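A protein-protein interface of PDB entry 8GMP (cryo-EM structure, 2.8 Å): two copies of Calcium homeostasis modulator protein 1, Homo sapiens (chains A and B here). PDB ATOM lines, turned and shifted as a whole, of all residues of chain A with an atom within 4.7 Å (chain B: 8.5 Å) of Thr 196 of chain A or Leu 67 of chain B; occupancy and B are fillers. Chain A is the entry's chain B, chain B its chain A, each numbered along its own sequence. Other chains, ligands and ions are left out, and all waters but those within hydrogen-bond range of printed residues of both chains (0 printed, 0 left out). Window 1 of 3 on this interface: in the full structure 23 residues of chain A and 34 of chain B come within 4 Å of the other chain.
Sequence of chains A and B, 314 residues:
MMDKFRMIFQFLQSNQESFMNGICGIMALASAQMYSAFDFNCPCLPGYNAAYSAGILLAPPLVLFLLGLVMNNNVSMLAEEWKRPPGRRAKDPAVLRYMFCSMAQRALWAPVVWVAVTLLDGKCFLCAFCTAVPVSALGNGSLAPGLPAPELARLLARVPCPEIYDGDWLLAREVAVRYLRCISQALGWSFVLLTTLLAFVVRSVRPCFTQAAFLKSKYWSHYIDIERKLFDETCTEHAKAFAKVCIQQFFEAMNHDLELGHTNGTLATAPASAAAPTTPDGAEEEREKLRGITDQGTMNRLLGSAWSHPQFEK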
ATOM      1  N   VAL A 192      -2.797 -21.607  10.459  1.00  0.00           N
ATOM      2  CA  VAL A 192      -2.783 -21.371   9.019  1.00  0.00           C
ATOM      3  C   VAL A 192      -1.536 -20.601   8.609  1.00  0.00           C
ATOM      4  O   VAL A 192      -1.054 -20.741   7.479  1.00  0.00           O
ATOM      5  CB  VAL A 192      -4.065 -20.635   8.591  1.00  0.00           C
ATOM      6  CG1 VAL A 192      -4.027 -20.329   7.110  1.00  0.00           C
ATOM      7  CG2 VAL A 192      -5.284 -21.463   8.935  1.00  0.00           C
ATOM      8  N   LEU A 193      -0.996 -19.778   9.508  1.00  0.00           N
ATOM      9  CA  LEU A 193       0.207 -19.016   9.195  1.00  0.00           C
ATOM     10  C   LEU A 193       1.436 -19.912   9.212  1.00  0.00           C
ATOM     11  O   LEU A 193       2.182 -19.988   8.229  1.00  0.00           O
ATOM     12  CB  LEU A 193       0.365 -17.861  10.185  1.00  0.00           C
ATOM     13  CG  LEU A 193       1.305 -16.724   9.786  1.00  0.00           C
ATOM     14  CD1 LEU A 193       0.866 -16.099   8.476  1.00  0.00           C
ATOM     15  CD2 LEU A 193       1.365 -15.677  10.880  1.00  0.00           C
ATOM     16  N   LEU A 194       1.661 -20.607  10.328  1.00  0.00           N
ATOM     17  CA  LEU A 194       2.849 -21.442  10.461  1.00  0.00           C
ATOM     18  C   LEU A 194       2.817 -22.621   9.496  1.00  0.00           C
ATOM     19  O   LEU A 194       3.854 -23.225   9.207  1.00  0.00           O
ATOM     20  CB  LEU A 194       2.979 -21.929  11.902  1.00  0.00           C
ATOM     21  CG  LEU A 194       4.114 -22.905  12.202  1.00  0.00           C
ATOM     22  CD1 LEU A 194       4.777 -22.546  13.518  1.00  0.00           C
ATOM     23  CD2 LEU A 194       3.595 -24.330  12.237  1.00  0.00           C
ATOM     24  N   THR A 195       1.634 -22.966   8.989  1.00  0.00           N
ATOM     25  CA  THR A 195       1.531 -24.054   8.024  1.00  0.00           C
ATOM     26  C   THR A 195       1.764 -23.550   6.606  1.00  0.00           C
ATOM     27  O   THR A 195       2.275 -24.283   5.753  1.00  0.00           O
ATOM     28  CB  THR A 195       0.164 -24.728   8.144  1.00  0.00           C
ATOM     29  OG1 THR A 195       0.129 -25.524   9.333  1.00  0.00           O
ATOM     30  CG2 THR A 195      -0.100 -25.612   6.950  1.00  0.00           C
ATOM     31  N   THR A 196       1.398 -22.297   6.335  1.00  0.00           N
ATOM     32  CA  THR A 196       1.664 -21.718   5.022  1.00  0.00           C
ATOM     33  C   THR A 196       3.102 -21.228   4.924  1.00  0.00           C
ATOM     34  O   THR A 196       3.671 -21.156   3.830  1.00  0.00           O
ATOM     35  CB  THR A 196       0.691 -20.576   4.739  1.00  0.00           C
ATOM     36  OG1 THR A 196      -0.651 -21.027   4.950  1.00  0.00           O
ATOM     37  CG2 THR A 196       0.832 -20.108   3.305  1.00  0.00           C
ATOM     38  N   LEU A 197       3.706 -20.884   6.062  1.00  0.00           N
ATOM     39  CA  LEU A 197       5.112 -20.497   6.072  1.00  0.00           C
ATOM     40  C   LEU A 197       6.024 -21.712   5.990  1.00  0.00           C
ATOM     41  O   LEU A 197       7.243 -21.565   5.860  1.00  0.00           O
ATOM     42  CB  LEU A 197       5.416 -19.689   7.332  1.00  0.00           C
ATOM     43  CG  LEU A 197       6.791 -19.036   7.441  1.00  0.00           C
ATOM     44  CD1 LEU A 197       7.020 -18.083   6.284  1.00  0.00           C
ATOM     45  CD2 LEU A 197       6.918 -18.312   8.766  1.00  0.00           C
ATOM     46  N   LEU A 198       5.457 -22.915   6.072  1.00  0.00           N
ATOM     47  CA  LEU A 198       6.224 -24.144   5.936  1.00  0.00           C
ATOM     48  C   LEU A 198       6.076 -24.771   4.558  1.00  0.00           C
ATOM     49  O   LEU A 198       7.015 -25.417   4.085  1.00  0.00           O
ATOM     50  CB  LEU A 198       5.799 -25.144   7.011  1.00  0.00           C
ATOM     51  CG  LEU A 198       6.589 -26.447   7.094  1.00  0.00           C
ATOM     52  CD1 LEU A 198       8.042 -26.154   7.417  1.00  0.00           C
ATOM     53  CD2 LEU A 198       5.985 -27.359   8.145  1.00  0.00           C
ATOM     54  N   ALA A 199       4.926 -24.595   3.905  1.00  0.00           N
ATOM     55  CA  ALA A 199       4.783 -24.989   2.511  1.00  0.00           C
ATOM     56  C   ALA A 199       5.547 -24.061   1.578  1.00  0.00           C
ATOM     57  O   ALA A 199       5.740 -24.397   0.406  1.00  0.00           O
ATOM     58  CB  ALA A 199       3.306 -25.017   2.122  1.00  0.00           C
ATOM     59  N   PHE A 200       5.975 -22.900   2.074  1.00  0.00           N
ATOM     60  CA  PHE A 200       6.791 -21.985   1.283  1.00  0.00           C
ATOM     61  C   PHE A 200       8.256 -22.395   1.327  1.00  0.00           C
ATOM     62  O   PHE A 200       8.995 -22.219   0.352  1.00  0.00           O
ATOM     63  CB  PHE A 200       6.610 -20.557   1.803  1.00  0.00           C
ATOM     64  CG  PHE A 200       7.398 -19.526   1.051  1.00  0.00           C
ATOM     65  CD1 PHE A 200       7.012 -19.122  -0.212  1.00  0.00           C
ATOM     66  CD2 PHE A 200       8.523 -18.953   1.616  1.00  0.00           C
ATOM     67  CE1 PHE A 200       7.734 -18.172  -0.900  1.00  0.00           C
ATOM     68  CE2 PHE A 200       9.249 -18.003   0.932  1.00  0.00           C
ATOM     69  CZ  PHE A 200       8.854 -17.612  -0.328  1.00  0.00           C
ATOM     70  N   MET B  27      -7.956 -15.910  -6.929  1.00  0.00           N
ATOM     71  CA  MET B  27      -7.354 -15.516  -5.660  1.00  0.00           C
ATOM     72  C   MET B  27      -8.076 -14.312  -5.065  1.00  0.00           C
ATOM     73  O   MET B  27      -8.294 -14.237  -3.851  1.00  0.00           O
ATOM     74  CB  MET B  27      -5.867 -15.216  -5.857  1.00  0.00           C
ATOM     75  N   ALA B  30     -11.603 -15.506  -3.998  1.00  0.00           N
ATOM     76  CA  ALA B  30     -11.559 -16.252  -2.744  1.00  0.00           C
ATOM     77  C   ALA B  30     -11.168 -15.362  -1.573  1.00  0.00           C
ATOM     78  O   ALA B  30     -11.181 -15.813  -0.423  1.00  0.00           O
ATOM     79  CB  ALA B  30     -10.590 -17.428  -2.864  1.00  0.00           C
ATOM     80  N   MET B  34     -14.176 -15.327   1.270  1.00  0.00           N
ATOM     81  CA  MET B  34     -13.664 -15.901   2.505  1.00  0.00           C
ATOM     82  C   MET B  34     -13.899 -14.989   3.700  1.00  0.00           C
ATOM     83  O   MET B  34     -13.712 -15.422   4.843  1.00  0.00           O
ATOM     84  CB  MET B  34     -12.167 -16.198   2.364  1.00  0.00           C
ATOM     85  CG  MET B  34     -11.549 -16.960   3.524  1.00  0.00           C
ATOM     86  SD  MET B  34      -9.830 -17.405   3.209  1.00  0.00           S
ATOM     87  CE  MET B  34      -8.982 -15.966   3.855  1.00  0.00           C
ATOM     88  N   PRO B  60      -4.493 -12.570   7.997  1.00  0.00           N
ATOM     89  CA  PRO B  60      -4.989 -13.170   6.747  1.00  0.00           C
ATOM     90  C   PRO B  60      -4.553 -12.411   5.502  1.00  0.00           C
ATOM     91  O   PRO B  60      -4.509 -13.005   4.415  1.00  0.00           O
ATOM     92  CB  PRO B  60      -6.516 -13.140   6.915  1.00  0.00           C
ATOM     93  CG  PRO B  60      -6.770 -12.237   8.034  1.00  0.00           C
ATOM     94  CD  PRO B  60      -5.596 -12.267   8.921  1.00  0.00           C
ATOM     95  N   PRO B  61      -4.235 -11.099   5.581  1.00  0.00           N
ATOM     96  CA  PRO B  61      -3.537 -10.482   4.446  1.00  0.00           C
ATOM     97  C   PRO B  61      -2.157 -11.078   4.219  1.00  0.00           C
ATOM     98  O   PRO B  61      -1.752 -11.307   3.077  1.00  0.00           O
ATOM     99  CB  PRO B  61      -3.454  -9.007   4.848  1.00  0.00           C
ATOM    100  CG  PRO B  61      -4.653  -8.801   5.649  1.00  0.00           C
ATOM    101  CD  PRO B  61      -4.828 -10.060   6.445  1.00  0.00           C
ATOM    102  N   LEU B  62      -1.426 -11.332   5.305  1.00  0.00           N
ATOM    103  CA  LEU B  62      -0.092 -11.907   5.184  1.00  0.00           C
ATOM    104  C   LEU B  62      -0.144 -13.355   4.712  1.00  0.00           C
ATOM    105  O   LEU B  62       0.844 -13.870   4.181  1.00  0.00           O
ATOM    106  CB  LEU B  62       0.633 -11.806   6.525  1.00  0.00           C
ATOM    107  CG  LEU B  62       2.149 -11.990   6.554  1.00  0.00           C
ATOM    108  CD1 LEU B  62       2.734 -11.235   7.726  1.00  0.00           C
ATOM    109  CD2 LEU B  62       2.513 -13.450   6.645  1.00  0.00           C
ATOM    110  N   VAL B  63      -1.283 -14.024   4.895  1.00  0.00           N
ATOM    111  CA  VAL B  63      -1.413 -15.415   4.464  1.00  0.00           C
ATOM    112  C   VAL B  63      -1.761 -15.480   2.984  1.00  0.00           C
ATOM    113  O   VAL B  63      -1.394 -16.428   2.282  1.00  0.00           O
ATOM    114  CB  VAL B  63      -2.460 -16.145   5.326  1.00  0.00           C
ATOM    115  CG1 VAL B  63      -3.022 -17.346   4.591  1.00  0.00           C
ATOM    116  CG2 VAL B  63      -1.853 -16.569   6.651  1.00  0.00           C
ATOM    117  N   LEU B  64      -2.476 -14.472   2.483  1.00  0.00           N
ATOM    118  CA  LEU B  64      -2.819 -14.440   1.067  1.00  0.00           C
ATOM    119  C   LEU B  64      -1.650 -13.983   0.208  1.00  0.00           C
ATOM    120  O   LEU B  64      -1.663 -14.205  -1.008  1.00  0.00           O
ATOM    121  CB  LEU B  64      -4.022 -13.524   0.839  1.00  0.00           C
ATOM    122  CG  LEU B  64      -5.377 -13.993   1.367  1.00  0.00           C
ATOM    123  CD1 LEU B  64      -6.242 -12.800   1.726  1.00  0.00           C
ATOM    124  CD2 LEU B  64      -6.075 -14.870   0.347  1.00  0.00           C
ATOM    125  N   PHE B  65      -0.648 -13.343   0.808  1.00  0.00           N
ATOM    126  CA  PHE B  65       0.555 -12.970   0.073  1.00  0.00           C
ATOM    127  C   PHE B  65       1.448 -14.184  -0.152  1.00  0.00           C
ATOM    128  O   PHE B  65       1.852 -14.474  -1.284  1.00  0.00           O
ATOM    129  CB  PHE B  65       1.303 -11.874   0.832  1.00  0.00           C
ATOM    130  CG  PHE B  65       2.516 -11.357   0.118  1.00  0.00           C
ATOM    131  CD1 PHE B  65       2.404 -10.768  -1.128  1.00  0.00           C
ATOM    132  CD2 PHE B  65       3.766 -11.446   0.698  1.00  0.00           C
ATOM    133  CE1 PHE B  65       3.516 -10.287  -1.784  1.00  0.00           C
ATOM    134  CE2 PHE B  65       4.882 -10.967   0.046  1.00  0.00           C
ATOM    135  CZ  PHE B  65       4.756 -10.386  -1.195  1.00  0.00           C
ATOM    136  N   LEU B  66       1.761 -14.912   0.921  1.00  0.00           N
ATOM    137  CA  LEU B  66       2.570 -16.118   0.793  1.00  0.00           C
ATOM    138  C   LEU B  66       1.858 -17.194  -0.013  1.00  0.00           C
ATOM    139  O   LEU B  66       2.512 -18.045  -0.623  1.00  0.00           O
ATOM    140  CB  LEU B  66       2.939 -16.651   2.176  1.00  0.00           C
ATOM    141  CG  LEU B  66       4.186 -16.051   2.821  1.00  0.00           C
ATOM    142  CD1 LEU B  66       3.972 -14.593   3.148  1.00  0.00           C
ATOM    143  CD2 LEU B  66       4.543 -16.823   4.073  1.00  0.00           C
ATOM    144  N   LEU B  67       0.529 -17.178  -0.029  1.00  0.00           N
ATOM    145  CA  LEU B  67      -0.222 -18.156  -0.806  1.00  0.00           C
ATOM    146  C   LEU B  67      -0.331 -17.781  -2.276  1.00  0.00           C
ATOM    147  O   LEU B  67      -0.983 -18.501  -3.037  1.00  0.00           O
ATOM    148  CB  LEU B  67      -1.620 -18.332  -0.215  1.00  0.00           C
ATOM    149  CG  LEU B  67      -2.295 -19.682  -0.450  1.00  0.00           C
ATOM    150  CD1 LEU B  67      -1.681 -20.740   0.449  1.00  0.00           C
ATOM    151  CD2 LEU B  67      -3.793 -19.582  -0.222  1.00  0.00           C
ATOM    152  N   GLY B  68       0.278 -16.673  -2.687  1.00  0.00           N
ATOM    153  CA  GLY B  68       0.330 -16.300  -4.086  1.00  0.00           C
ATOM    154  C   GLY B  68       1.726 -16.483  -4.638  1.00  0.00           C
ATOM    155  O   GLY B  68       1.907 -16.732  -5.832  1.00  0.00           O
ATOM    156  N   LEU B  69       2.726 -16.347  -3.766  1.00  0.00           N
ATOM    157  CA  LEU B  69       4.095 -16.671  -4.148  1.00  0.00           C
ATOM    158  C   LEU B  69       4.270 -18.175  -4.310  1.00  0.00           C
ATOM    159  O   LEU B  69       4.884 -18.643  -5.274  1.00  0.00           O
ATOM    160  CB  LEU B  69       5.070 -16.123  -3.109  1.00  0.00           C
ATOM    161  CG  LEU B  69       5.126 -14.607  -2.947  1.00  0.00           C
ATOM    162  CD1 LEU B  69       6.286 -14.214  -2.057  1.00  0.00           C
ATOM    163  CD2 LEU B  69       5.239 -13.935  -4.297  1.00  0.00           C
ATOM    164  N   VAL B  70       3.740 -18.949  -3.361  1.00  0.00           N
ATOM    165  CA  VAL B  70       3.867 -20.401  -3.390  1.00  0.00           C
ATOM    166  C   VAL B  70       3.210 -21.019  -4.617  1.00  0.00           C
ATOM    167  O   VAL B  70       3.647 -22.076  -5.082  1.00  0.00           O
ATOM    168  CB  VAL B  70       3.278 -20.995  -2.091  1.00  0.00           C
ATOM    169  CG1 VAL B  70       2.941 -22.463  -2.266  1.00  0.00           C
ATOM    170  CG2 VAL B  70       4.246 -20.812  -0.940  1.00  0.00           C
ATOM    171  N   MET B  71       2.185 -20.375  -5.179  1.00  0.00           N
ATOM    172  CA  MET B  71       1.382 -21.058  -6.188  1.00  0.00           C
ATOM    173  C   MET B  71       1.577 -20.484  -7.587  1.00  0.00           C
ATOM    174  O   MET B  71       0.635 -20.483  -8.386  1.00  0.00           O
ATOM    175  CB  MET B  71      -0.094 -21.019  -5.800  1.00  0.00           C
ATOM    176  CG  MET B  71      -0.416 -21.843  -4.565  1.00  0.00           C
ATOM    177  SD  MET B  71      -2.158 -21.780  -4.111  1.00  0.00           S
ATOM    178  CE  MET B  71      -2.884 -22.762  -5.420  1.00  0.00           C
ATOM    179  N   ASN B  72       2.768 -19.988  -7.906  1.00  0.00           N
ATOM    180  CA  ASN B  72       3.146 -19.772  -9.295  1.00  0.00           C
ATOM    181  C   ASN B  72       4.429 -20.538  -9.602  1.00  0.00           C
ATOM    182  O   ASN B  72       5.276 -20.744  -8.728  1.00  0.00           O
ATOM    183  CB  ASN B  72       3.315 -18.282  -9.609  1.00  0.00           C
ATOM    184  CG  ASN B  72       4.414 -17.625  -8.801  1.00  0.00           C
ATOM    185  OD1 ASN B  72       5.002 -18.226  -7.908  1.00  0.00           O
ATOM    186  ND2 ASN B  72       4.703 -16.373  -9.128  1.00  0.00           N
ATOM    187  N   ARG B 106       1.467  -9.368  -8.460  1.00  0.00           N
ATOM    188  CA  ARG B 106       0.194 -10.066  -8.606  1.00  0.00           C
ATOM    189  C   ARG B 106      -0.246 -10.696  -7.290  1.00  0.00           C
ATOM    190  O   ARG B 106      -1.421 -11.042  -7.123  1.00  0.00           O
ATOM    191  CB  ARG B 106       0.288 -11.108  -9.717  1.00  0.00           C
ATOM    192  CG  ARG B 106       1.630 -11.133 -10.417  1.00  0.00           C
ATOM    193  CD  ARG B 106       1.589 -12.057 -11.619  1.00  0.00           C
ATOM    194  NE  ARG B 106       0.653 -11.562 -12.625  1.00  0.00           N
ATOM    195  CZ  ARG B 106       0.270 -12.244 -13.700  1.00  0.00           C
ATOM    196  NH1 ARG B 106       0.751 -13.460 -13.926  1.00  0.00           N
ATOM    197  NH2 ARG B 106      -0.589 -11.700 -14.555  1.00  0.00           N
ATOM    198  N   ALA B 107       0.681 -10.851  -6.343  1.00  0.00           N
ATOM    199  CA  ALA B 107       0.322 -11.364  -5.025  1.00  0.00           C
ATOM    200  C   ALA B 107      -0.312 -10.278  -4.165  1.00  0.00           C
ATOM    201  O   ALA B 107      -0.769 -10.542  -3.048  1.00  0.00           O
ATOM    202  CB  ALA B 107       1.556 -11.946  -4.333  1.00  0.00           C
ATOM    203  N   ALA B 110      -5.088  -9.761  -3.503  1.00  0.00           N
ATOM    204  CA  ALA B 110      -5.875 -10.244  -2.378  1.00  0.00           C
ATOM    205  C   ALA B 110      -5.570  -9.488  -1.088  1.00  0.00           C
ATOM    206  O   ALA B 110      -6.503  -9.115  -0.367  1.00  0.00           O
ATOM    207  CB  ALA B 110      -5.640 -11.742  -2.184  1.00  0.00           C
ATOM    208  N   PRO B 111      -4.299  -9.258  -0.742  1.00  0.00           N
ATOM    209  CA  PRO B 111      -4.009  -8.447   0.452  1.00  0.00           C
ATOM    210  C   PRO B 111      -4.601  -7.047   0.418  1.00  0.00           C
ATOM    211  O   PRO B 111      -4.796  -6.444   1.480  1.00  0.00           O
ATOM    212  CB  PRO B 111      -2.478  -8.407   0.469  1.00  0.00           C
ATOM    213  CG  PRO B 111      -2.081  -9.667  -0.159  1.00  0.00           C
ATOM    214  CD  PRO B 111      -3.093  -9.949  -1.227  1.00  0.00           C
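O of Val 192 of chain A lies within hydrogen-bond range of OG1 of Thr 196 of chain A.
Among the printed residues, pairs that only touch across the chains: Leu 193 of chain A with Val 63 of chain B (3.3 Å), Phe 200 of chain A with Val 70 of chain B (3.3 Å), Leu 197 of chain A with Leu 66 of chain B (3.6 Å), Leu 193 of chain A with Leu 62 of chain B (3.6 Å) and Thr 196 of chain A with Leu 67 of chain B (3.9 Å).
Of the printed residues of chain B, Thr 196 of chain A touches Leu 67 (3.9 Å).
Leu 67 of chain B touches just one residue of chain A: Thr 196.
Printed residues of chain A within 4 Å of Leu 62 of chain B: Leu 193.
Of the printed residues of chain B, Leu 193 of chain A touches Leu 62 (3.6 Å) and Val 63 (3.3 Å).
The nearest printed residue of chain A that does not touch Leu 67 of chain B is Phe 200 of chain A (6.8 Å).
The nearest printed residue of chain B that does not touch Phe 200 of chain A is Leu 69 of chain B (4.02 Å).
Hydrophobic or aromatic side chains of chain A that line the printed part of chain B: Leu 193, Leu 197 and Phe 200.
Of the 20 printed residues of chain B, 5 touch a printed residue of chain A.
Hydrophobic or aromatic side chains of chain B that line the printed part of chain A: Leu 62, Val 63, Leu 66, Leu 67 and Val 70.
Among the printed residues, no Asp or Glu carboxylate lies within 4 Å of a Lys or Arg side-chain nitrogen of the other chain.
No position is printed for both chains.
Of the 5 pairs that touch across the chains among the printed residues, none has its exchanged pair printed and touching as well.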
